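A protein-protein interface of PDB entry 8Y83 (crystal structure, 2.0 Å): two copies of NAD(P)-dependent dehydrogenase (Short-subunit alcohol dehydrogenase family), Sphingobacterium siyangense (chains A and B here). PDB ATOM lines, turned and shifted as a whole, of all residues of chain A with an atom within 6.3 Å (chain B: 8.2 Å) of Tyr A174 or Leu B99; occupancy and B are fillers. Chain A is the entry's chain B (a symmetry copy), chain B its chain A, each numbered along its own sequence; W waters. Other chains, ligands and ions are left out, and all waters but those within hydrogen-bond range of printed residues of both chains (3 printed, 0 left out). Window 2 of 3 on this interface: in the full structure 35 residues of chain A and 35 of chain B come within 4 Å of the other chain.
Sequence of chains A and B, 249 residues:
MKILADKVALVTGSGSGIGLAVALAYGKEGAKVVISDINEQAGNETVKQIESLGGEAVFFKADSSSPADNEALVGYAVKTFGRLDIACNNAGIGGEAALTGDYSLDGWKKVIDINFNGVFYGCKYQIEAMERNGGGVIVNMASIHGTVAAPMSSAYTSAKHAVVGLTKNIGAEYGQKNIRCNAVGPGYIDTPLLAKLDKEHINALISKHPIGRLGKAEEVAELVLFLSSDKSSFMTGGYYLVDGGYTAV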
ATOM      1  N   ILE A 127      19.283 -29.888  29.018  1.00  0.00           N
ATOM      2  CA  ILE A 127      19.664 -28.649  29.692  1.00  0.00           C
ATOM      3  C   ILE A 127      20.100 -28.941  31.132  1.00  0.00           C
ATOM      4  O   ILE A 127      21.100 -28.398  31.620  1.00  0.00           O
ATOM      5  CB  ILE A 127      18.525 -27.606  29.633  1.00  0.00           C
ATOM      6  CG1 ILE A 127      18.413 -27.020  28.223  1.00  0.00           C
ATOM      7  CG2 ILE A 127      18.680 -26.491  30.674  1.00  0.00           C
ATOM      8  CD1 ILE A 127      17.116 -26.310  27.953  1.00  0.00           C
ATOM      9  N   GLU A 131      23.805 -27.950  32.552  1.00  0.00           N
ATOM     10  CA  GLU A 131      24.044 -27.007  33.644  1.00  0.00           C
ATOM     11  C   GLU A 131      24.967 -27.587  34.722  1.00  0.00           C
ATOM     12  O   GLU A 131      25.656 -26.834  35.379  1.00  0.00           O
ATOM     13  CB  GLU A 131      22.789 -26.638  34.439  1.00  0.00           C
ATOM     14  CG  GLU A 131      21.796 -25.802  33.645  1.00  0.00           C
ATOM     15  CD  GLU A 131      20.436 -25.688  34.324  1.00  0.00           C
ATOM     16  OE1 GLU A 131      19.999 -24.532  34.374  1.00  0.00           O
ATOM     17  OE2 GLU A 131      19.826 -26.673  34.811  1.00  0.00           O
ATOM     18  N   ASN A 169      13.629 -19.560  22.428  1.00  0.00           N
ATOM     19  CA  ASN A 169      13.439 -19.422  23.856  1.00  0.00           C
ATOM     20  C   ASN A 169      14.661 -19.939  24.631  1.00  0.00           C
ATOM     21  O   ASN A 169      15.131 -19.271  25.554  1.00  0.00           O
ATOM     22  CB  ASN A 169      12.115 -20.066  24.312  1.00  0.00           C
ATOM     23  CG  ASN A 169      11.183 -19.054  24.905  1.00  0.00           C
ATOM     24  OD1 ASN A 169      10.553 -18.287  24.178  1.00  0.00           O
ATOM     25  ND2 ASN A 169      11.080 -18.990  26.219  1.00  0.00           N
ATOM     26  N   ILE A 170      15.165 -21.129  24.278  1.00  0.00           N
ATOM     27  CA  ILE A 170      16.304 -21.695  24.999  1.00  0.00           C
ATOM     28  C   ILE A 170      17.533 -20.807  24.813  1.00  0.00           C
ATOM     29  O   ILE A 170      18.239 -20.477  25.759  1.00  0.00           O
ATOM     30  CB  ILE A 170      16.564 -23.149  24.552  1.00  0.00           C
ATOM     31  CG1 ILE A 170      15.369 -24.037  24.858  1.00  0.00           C
ATOM     32  CG2 ILE A 170      17.859 -23.701  25.165  1.00  0.00           C
ATOM     33  CD1 ILE A 170      15.413 -25.440  24.259  1.00  0.00           C
ATOM     34  N   GLY A 171      17.810 -20.436  23.559  1.00  0.00           N
ATOM     35  CA  GLY A 171      18.966 -19.603  23.288  1.00  0.00           C
ATOM     36  C   GLY A 171      18.936 -18.306  24.079  1.00  0.00           C
ATOM     37  O   GLY A 171      19.950 -17.909  24.669  1.00  0.00           O
ATOM     38  N   ALA A 172      17.762 -17.666  24.112  1.00  0.00           N
ATOM     39  CA  ALA A 172      17.616 -16.407  24.816  1.00  0.00           C
ATOM     40  C   ALA A 172      17.735 -16.608  26.329  1.00  0.00           C
ATOM     41  O   ALA A 172      18.375 -15.798  27.009  1.00  0.00           O
ATOM     42  CB  ALA A 172      16.310 -15.755  24.424  1.00  0.00           C
ATOM     43  N   GLU A 173      17.177 -17.714  26.841  1.00  0.00           N
ATOM     44  CA  GLU A 173      17.095 -17.910  28.293  1.00  0.00           C
ATOM     45  C   GLU A 173      18.472 -18.232  28.889  1.00  0.00           C
ATOM     46  O   GLU A 173      18.793 -17.774  29.985  1.00  0.00           O
ATOM     47  CB  GLU A 173      16.171 -19.073  28.645  1.00  0.00           C
ATOM     48  CG  GLU A 173      14.683 -18.720  28.650  1.00  0.00           C
ATOM     49  CD  GLU A 173      13.754 -19.906  28.765  1.00  0.00           C
ATOM     50  OE1 GLU A 173      14.233 -21.076  28.779  1.00  0.00           O
ATOM     51  OE2 GLU A 173      12.519 -19.646  28.689  1.00  0.00           O
ATOM     52  N   TYR A 174      19.263 -19.065  28.192  1.00  0.00           N
ATOM     53  CA  TYR A 174      20.497 -19.622  28.739  1.00  0.00           C
ATOM     54  C   TYR A 174      21.747 -18.965  28.170  1.00  0.00           C
ATOM     55  O   TYR A 174      22.842 -19.505  28.317  1.00  0.00           O
ATOM     56  CB  TYR A 174      20.485 -21.115  28.418  1.00  0.00           C
ATOM     57  CG  TYR A 174      19.473 -21.849  29.283  1.00  0.00           C
ATOM     58  CD1 TYR A 174      19.819 -22.308  30.553  1.00  0.00           C
ATOM     59  CD2 TYR A 174      18.168 -22.041  28.861  1.00  0.00           C
ATOM     60  CE1 TYR A 174      18.896 -22.960  31.362  1.00  0.00           C
ATOM     61  CE2 TYR A 174      17.244 -22.705  29.649  1.00  0.00           C
ATOM     62  CZ  TYR A 174      17.603 -23.153  30.918  1.00  0.00           C
ATOM     63  OH  TYR A 174      16.695 -23.833  31.705  1.00  0.00           O
ATOM     64  N   GLY A 175      21.582 -17.796  27.537  1.00  0.00           N
ATOM     65  CA  GLY A 175      22.700 -17.070  26.950  1.00  0.00           C
ATOM     66  C   GLY A 175      23.848 -16.897  27.940  1.00  0.00           C
ATOM     67  O   GLY A 175      24.983 -17.209  27.613  1.00  0.00           O
ATOM     68  N   GLN A 176      23.527 -16.426  29.150  1.00  0.00           N
ATOM     69  CA  GLN A 176      24.536 -16.215  30.175  1.00  0.00           C
ATOM     70  C   GLN A 176      24.797 -17.462  31.017  1.00  0.00           C
ATOM     71  O   GLN A 176      25.530 -17.371  31.985  1.00  0.00           O
ATOM     72  CB  GLN A 176      24.135 -15.061  31.076  1.00  0.00           C
ATOM     73  CG  GLN A 176      23.892 -13.775  30.310  1.00  0.00           C
ATOM     74  CD  GLN A 176      23.652 -12.618  31.245  1.00  0.00           C
ATOM     75  OE1 GLN A 176      22.518 -12.286  31.585  1.00  0.00           O
ATOM     76  NE2 GLN A 176      24.729 -12.008  31.687  1.00  0.00           N
ATOM     77  N   LYS A 177      24.248 -18.631  30.664  1.00  0.00           N
ATOM     78  CA  LYS A 177      24.504 -19.839  31.435  1.00  0.00           C
ATOM     79  C   LYS A 177      25.336 -20.807  30.601  1.00  0.00           C
ATOM     80  O   LYS A 177      25.400 -21.975  30.890  1.00  0.00           O
ATOM     81  CB  LYS A 177      23.201 -20.510  31.891  1.00  0.00           C
ATOM     82  CG  LYS A 177      22.146 -19.644  32.613  1.00  0.00           C
ATOM     83  CD  LYS A 177      22.261 -19.440  34.120  1.00  0.00           C
ATOM     84  CE  LYS A 177      22.624 -18.053  34.586  1.00  0.00           C
ATOM     85  NZ  LYS A 177      21.522 -17.095  34.427  1.00  0.00           N
ATOM     86  N   ASN A 178      25.926 -20.322  29.517  1.00  0.00           N
ATOM     87  CA  ASN A 178      26.805 -21.088  28.663  1.00  0.00           C
ATOM     88  C   ASN A 178      26.136 -22.301  28.018  1.00  0.00           C
ATOM     89  O   ASN A 178      26.796 -23.320  27.823  1.00  0.00           O
ATOM     90  CB  ASN A 178      28.051 -21.519  29.420  1.00  0.00           C
ATOM     91  CG  ASN A 178      29.170 -21.873  28.474  1.00  0.00           C
ATOM     92  OD1 ASN A 178      29.338 -21.243  27.422  1.00  0.00           O
ATOM     93  ND2 ASN A 178      29.940 -22.888  28.818  1.00  0.00           N
ATOM     94  N   ILE A 179      24.835 -22.199  27.699  1.00  0.00           N
ATOM     95  CA  ILE A 179      24.190 -23.182  26.858  1.00  0.00           C
ATOM     96  C   ILE A 179      23.696 -22.450  25.614  1.00  0.00           C
ATOM     97  O   ILE A 179      22.976 -21.465  25.736  1.00  0.00           O
ATOM     98  CB  ILE A 179      23.063 -23.909  27.626  1.00  0.00           C
ATOM     99  CG1 ILE A 179      23.633 -24.665  28.837  1.00  0.00           C
ATOM    100  CG2 ILE A 179      22.272 -24.827  26.684  1.00  0.00           C
ATOM    101  CD1 ILE A 179      22.605 -25.153  29.841  1.00  0.00           C
ATOM    102  N   ARG A 180      24.038 -22.986  24.438  1.00  0.00           N
ATOM    103  CA  ARG A 180      23.606 -22.418  23.172  1.00  0.00           C
ATOM    104  C   ARG A 180      22.611 -23.374  22.535  1.00  0.00           C
ATOM    105  O   ARG A 180      22.731 -24.587  22.681  1.00  0.00           O
ATOM    106  CB  ARG A 180      24.757 -22.151  22.194  1.00  0.00           C
ATOM    107  CG  ARG A 180      25.725 -21.095  22.701  1.00  0.00           C
ATOM    108  CD  ARG A 180      26.782 -20.727  21.654  1.00  0.00           C
ATOM    109  NE  ARG A 180      27.671 -21.833  21.306  1.00  0.00           N
ATOM    110  CZ  ARG A 180      27.682 -22.561  20.212  1.00  0.00           C
ATOM    111  NH1 ARG A 180      26.784 -22.365  19.284  1.00  0.00           N
ATOM    112  NH2 ARG A 180      28.621 -23.473  20.018  1.00  0.00           N
ATOM    113  N   GLU B  96       2.805 -21.171  33.077  1.00  0.00           N
ATOM    114  CA  GLU B  96       3.750 -20.889  34.163  1.00  0.00           C
ATOM    115  C   GLU B  96       5.005 -20.224  33.604  1.00  0.00           C
ATOM    116  O   GLU B  96       5.334 -20.403  32.431  1.00  0.00           O
ATOM    117  CB  GLU B  96       4.164 -22.184  34.870  1.00  0.00           C
ATOM    118  CG  GLU B  96       4.984 -23.126  33.999  1.00  0.00           C
ATOM    119  CD  GLU B  96       5.268 -24.517  34.545  1.00  0.00           C
ATOM    120  OE1 GLU B  96       6.433 -24.988  34.633  1.00  0.00           O
ATOM    121  OE2 GLU B  96       4.289 -25.151  34.891  1.00  0.00           O
ATOM    122  N   ALA B  97       5.673 -19.466  34.476  1.00  0.00           N
ATOM    123  CA  ALA B  97       6.954 -18.832  34.233  1.00  0.00           C
ATOM    124  C   ALA B  97       8.082 -19.652  34.884  1.00  0.00           C
ATOM    125  O   ALA B  97       8.151 -19.814  36.102  1.00  0.00           O
ATOM    126  CB  ALA B  97       6.907 -17.413  34.746  1.00  0.00           C
ATOM    127  N   ALA B  98       8.946 -20.214  34.033  1.00  0.00           N
ATOM    128  CA  ALA B  98      10.096 -21.027  34.418  1.00  0.00           C
ATOM    129  C   ALA B  98      11.001 -21.181  33.191  1.00  0.00           C
ATOM    130  O   ALA B  98      10.504 -21.208  32.073  1.00  0.00           O
ATOM    131  CB  ALA B  98       9.644 -22.395  34.927  1.00  0.00           C
ATOM    132  N   LEU B  99      12.316 -21.239  33.412  1.00  0.00           N
ATOM    133  CA  LEU B  99      13.262 -21.605  32.365  1.00  0.00           C
ATOM    134  C   LEU B  99      12.918 -22.978  31.816  1.00  0.00           C
ATOM    135  O   LEU B  99      12.410 -23.851  32.528  1.00  0.00           O
ATOM    136  CB  LEU B  99      14.679 -21.573  32.921  1.00  0.00           C
ATOM    137  CG  LEU B  99      15.160 -20.246  33.502  1.00  0.00           C
ATOM    138  CD1 LEU B  99      16.509 -20.482  34.136  1.00  0.00           C
ATOM    139  CD2 LEU B  99      15.228 -19.168  32.429  1.00  0.00           C
ATOM    140  N   THR B 100      13.266 -23.184  30.542  1.00  0.00           N
ATOM    141  CA  THR B 100      12.868 -24.372  29.814  1.00  0.00           C
ATOM    142  C   THR B 100      13.247 -25.635  30.579  1.00  0.00           C
ATOM    143  O   THR B 100      12.452 -26.568  30.676  1.00  0.00           O
ATOM    144  CB  THR B 100      13.522 -24.350  28.429  1.00  0.00           C
ATOM    145  OG1 THR B 100      13.092 -23.219  27.671  1.00  0.00           O
ATOM    146  CG2 THR B 100      13.126 -25.540  27.599  1.00  0.00           C
ATOM    147  N   GLY B 101      14.495 -25.684  31.064  1.00  0.00           N
ATOM    148  CA  GLY B 101      14.987 -26.818  31.824  1.00  0.00           C
ATOM    149  C   GLY B 101      14.132 -27.099  33.059  1.00  0.00           C
ATOM    150  O   GLY B 101      13.991 -28.244  33.458  1.00  0.00           O
ATOM    151  N   ASP B 102      13.507 -26.060  33.609  1.00  0.00           N
ATOM    152  CA  ASP B 102      12.735 -26.200  34.832  1.00  0.00           C
ATOM    153  C   ASP B 102      11.238 -26.268  34.543  1.00  0.00           C
ATOM    154  O   ASP B 102      10.460 -26.247  35.482  1.00  0.00           O
ATOM    155  CB  ASP B 102      13.042 -25.063  35.790  1.00  0.00           C
ATOM    156  CG  ASP B 102      14.514 -24.850  36.127  1.00  0.00           C
ATOM    157  OD1 ASP B 102      15.186 -25.853  36.263  1.00  0.00           O
ATOM    158  OD2 ASP B 102      14.961 -23.677  36.179  1.00  0.00           O
ATOM    159  N   TYR B 103      10.811 -26.307  33.266  1.00  0.00           N
ATOM    160  CA  TYR B 103       9.402 -26.164  32.923  1.00  0.00           C
ATOM    161  C   TYR B 103       8.698 -27.489  33.261  1.00  0.00           C
ATOM    162  O   TYR B 103       9.200 -28.556  32.905  1.00  0.00           O
ATOM    163  CB  TYR B 103       9.270 -25.748  31.444  1.00  0.00           C
ATOM    164  CG  TYR B 103       8.027 -24.929  31.153  1.00  0.00           C
ATOM    165  CD1 TYR B 103       6.784 -25.542  31.003  1.00  0.00           C
ATOM    166  CD2 TYR B 103       8.073 -23.551  31.098  1.00  0.00           C
ATOM    167  CE1 TYR B 103       5.633 -24.804  30.787  1.00  0.00           C
ATOM    168  CE2 TYR B 103       6.931 -22.802  30.840  1.00  0.00           C
ATOM    169  CZ  TYR B 103       5.700 -23.431  30.715  1.00  0.00           C
ATOM    170  OH  TYR B 103       4.546 -22.755  30.515  1.00  0.00           O
ATOM    171  N   SER B 104       7.534 -27.448  33.934  1.00  0.00           N
ATOM    172  CA  SER B 104       6.883 -28.698  34.353  1.00  0.00           C
ATOM    173  C   SER B 104       6.293 -29.426  33.157  1.00  0.00           C
ATOM    174  O   SER B 104       5.838 -28.799  32.190  1.00  0.00           O
ATOM    175  CB  SER B 104       5.823 -28.502  35.433  1.00  0.00           C
ATOM    176  OG  SER B 104       4.688 -27.798  34.938  1.00  0.00           O
ATOM    177  N   ALA B 150       9.832 -15.429  24.364  1.00  0.00           N
ATOM    178  CA  ALA B 150       9.338 -14.889  25.611  1.00  0.00           C
ATOM    179  C   ALA B 150      10.051 -15.657  26.731  1.00  0.00           C
ATOM    180  O   ALA B 150       9.610 -16.744  27.115  1.00  0.00           O
ATOM    181  CB  ALA B 150       7.855 -15.079  25.663  1.00  0.00           C
ATOM    182  N   PRO B 151      11.235 -15.193  27.195  1.00  0.00           N
ATOM    183  CA  PRO B 151      12.001 -15.945  28.203  1.00  0.00           C
ATOM    184  C   PRO B 151      11.117 -16.305  29.394  1.00  0.00           C
ATOM    185  O   PRO B 151      10.355 -15.446  29.857  1.00  0.00           O
ATOM    186  CB  PRO B 151      13.147 -14.977  28.576  1.00  0.00           C
ATOM    187  CG  PRO B 151      13.331 -14.110  27.306  1.00  0.00           C
ATOM    188  CD  PRO B 151      11.900 -13.942  26.784  1.00  0.00           C
ATOM    189  N   MET B 152      11.217 -17.582  29.814  1.00  0.00           N
ATOM    190  CA  MET B 152      10.446 -18.181  30.901  1.00  0.00           C
ATOM    191  C   MET B 152       9.068 -18.678  30.445  1.00  0.00           C
ATOM    192  O   MET B 152       8.309 -19.268  31.226  1.00  0.00           O
ATOM    193  CB  MET B 152      10.250 -17.221  32.081  1.00  0.00           C
ATOM    194  CG  MET B 152      11.523 -16.531  32.510  1.00  0.00           C
ATOM    195  SD  MET B 152      12.214 -17.279  33.986  1.00  0.00           S
ATOM    196  CE  MET B 152      10.951 -17.068  35.246  1.00  0.00           C
ATOM    197  N   SER B 153       8.734 -18.493  29.169  1.00  0.00           N
ATOM    198  CA  SER B 153       7.465 -18.995  28.663  1.00  0.00           C
ATOM    199  C   SER B 153       7.679 -19.812  27.400  1.00  0.00           C
ATOM    200  O   SER B 153       7.025 -19.543  26.396  1.00  0.00           O
ATOM    201  CB  SER B 153       6.517 -17.882  28.361  1.00  0.00           C
ATOM    202  OG  SER B 153       6.368 -16.993  29.453  1.00  0.00           O
ATOM    203  N   SER B 154       8.545 -20.827  27.456  1.00  0.00           N
ATOM    204  CA  SER B 154       8.842 -21.652  26.288  1.00  0.00           C
ATOM    205  C   SER B 154       7.610 -22.355  25.716  1.00  0.00           C
ATOM    206  O   SER B 154       7.508 -22.535  24.489  1.00  0.00           O
ATOM    207  CB  SER B 154       9.956 -22.623  26.607  1.00  0.00           C
ATOM    208  OG  SER B 154       9.516 -23.426  27.699  1.00  0.00           O
ATOM    209  N   ALA B 155       6.689 -22.841  26.565  1.00  0.00           N
ATOM    210  CA  ALA B 155       5.534 -23.541  26.008  1.00  0.00           C
ATOM    211  C   ALA B 155       4.639 -22.578  25.231  1.00  0.00           C
ATOM    212  O   ALA B 155       4.133 -22.921  24.175  1.00  0.00           O
ATOM    213  CB  ALA B 155       4.735 -24.287  27.076  1.00  0.00           C
HETATM  214  O   HOH W   1      10.517 -21.555  29.465  1.00  0.00           O
HETATM  215  O   HOH W   2      17.417 -27.281  35.008  1.00  0.00           O
HETATM  216  O   HOH W   3      17.264 -24.583  34.102  1.00  0.00           O
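Water W2 bridges the side-chain carboxylate (OE2) of Glu A131 and the side-chain carboxylate (OD1) of Asp B102. Water W3 lies within hydrogen-bond range of the side-chain hydroxyl (OH) of Tyr A174 (2.6 Å), the side-chain carboxylate (OE1) of Glu A131 (2.7 Å) and the side-chain carboxylate (OD2) of Asp B102 (3.2 Å). Water W1 lies within hydrogen-bond range of the backbone carbonyl oxygen of Ala B98 (2.6 Å), the side-chain hydroxyl of Ser B154 (2.8 Å), the side-chain carboxylate of Glu A173 (2.9 Å) and the backbone NH of Thr B100 (3.4 Å).
Hydrophobic or aromatic side chains of chain B within 4 Å of the printed part of chain A: Leu B99. Along chain B the printed residues that touch a printed residue of chain A span positions 99 to 154. Of the 14 printed residues of chain A, 5 touch a printed residue of chain B.
The backbone carbonyl oxygen (O) of Tyr A174 lies within hydrogen-bond range of the backbone NH (N) of Ile A179 (3.4 Å). The backbone NH (N) of Ala B98 is in hydrogen-bond range of the backbone carbonyl oxygen (O) of Met B152. ND2 of Asn A169 lies within hydrogen-bond range of OE2 of Glu A173, 2.9 Å away.
Among the printed residues, merely in contact across the chains: Ile A127 with Gly B101, Asn A169 with Pro B151, Asn A169 with Met B152, Asn A169 with Ser B153, Ile A170 with Thr B100, Glu A173 with Leu B99, Glu A173 with Pro B151, Glu A173 with Ser B153, Tyr A174 with Leu B99 and Tyr A174 with Thr B100.
Printed residues of chain B within 4 Å of Ile A127: Gly B101. Of chain B, only Leu B99 (3.3 Å), Thr B100 (3.7 Å) and Gly B101 (2.9 Å) come within 4 Å of Tyr A174. No residue of chain B comes within 4 Å of Gly A175. Of chain A, only Glu A173 and Tyr A174 come within 4 Å of Leu B99. Of the printed residues of chain A, Ser B153 touches Asn A169 (3.7 Å) and Glu A173 (3.99 Å). The nearest residue of chain B that does not touch Tyr A174 is Asp B102 (4.3 Å). The nearest residue of chain A that does not touch Leu B99 is Glu A131 (5.4 Å). The nearest printed residue of chain B that does not touch Glu A173 is Ala B98 (4.2 Å).
No position is printed for both chains. Of the 15 pairs that touch across the chains among the printed residues, none has its exchanged pair printed and touching as well.
The backbone NH (N) of Gly B101 is in hydrogen-bond range of the side-chain hydroxyl (OH) of Tyr A174, 2.9 Å away. The side-chain hydroxyl of Thr B100 is in hydrogen-bond range of the side-chain carboxylate of Glu A173 (2.7 Å). The backbone NH of Met B152 lies within hydrogen-bond range of the side-chain carboxylate of Glu A173. The backbone carbonyl oxygen (O) of Ala B150 sits at hydrogen-bond distance from the side-chain amide nitrogen (ND2) of Asn A169 (2.8 Å). The backbone NH (N) of Ser B154 lies close to the side-chain amide nitrogen (ND2) of Asn A169, at 3.4 Å.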
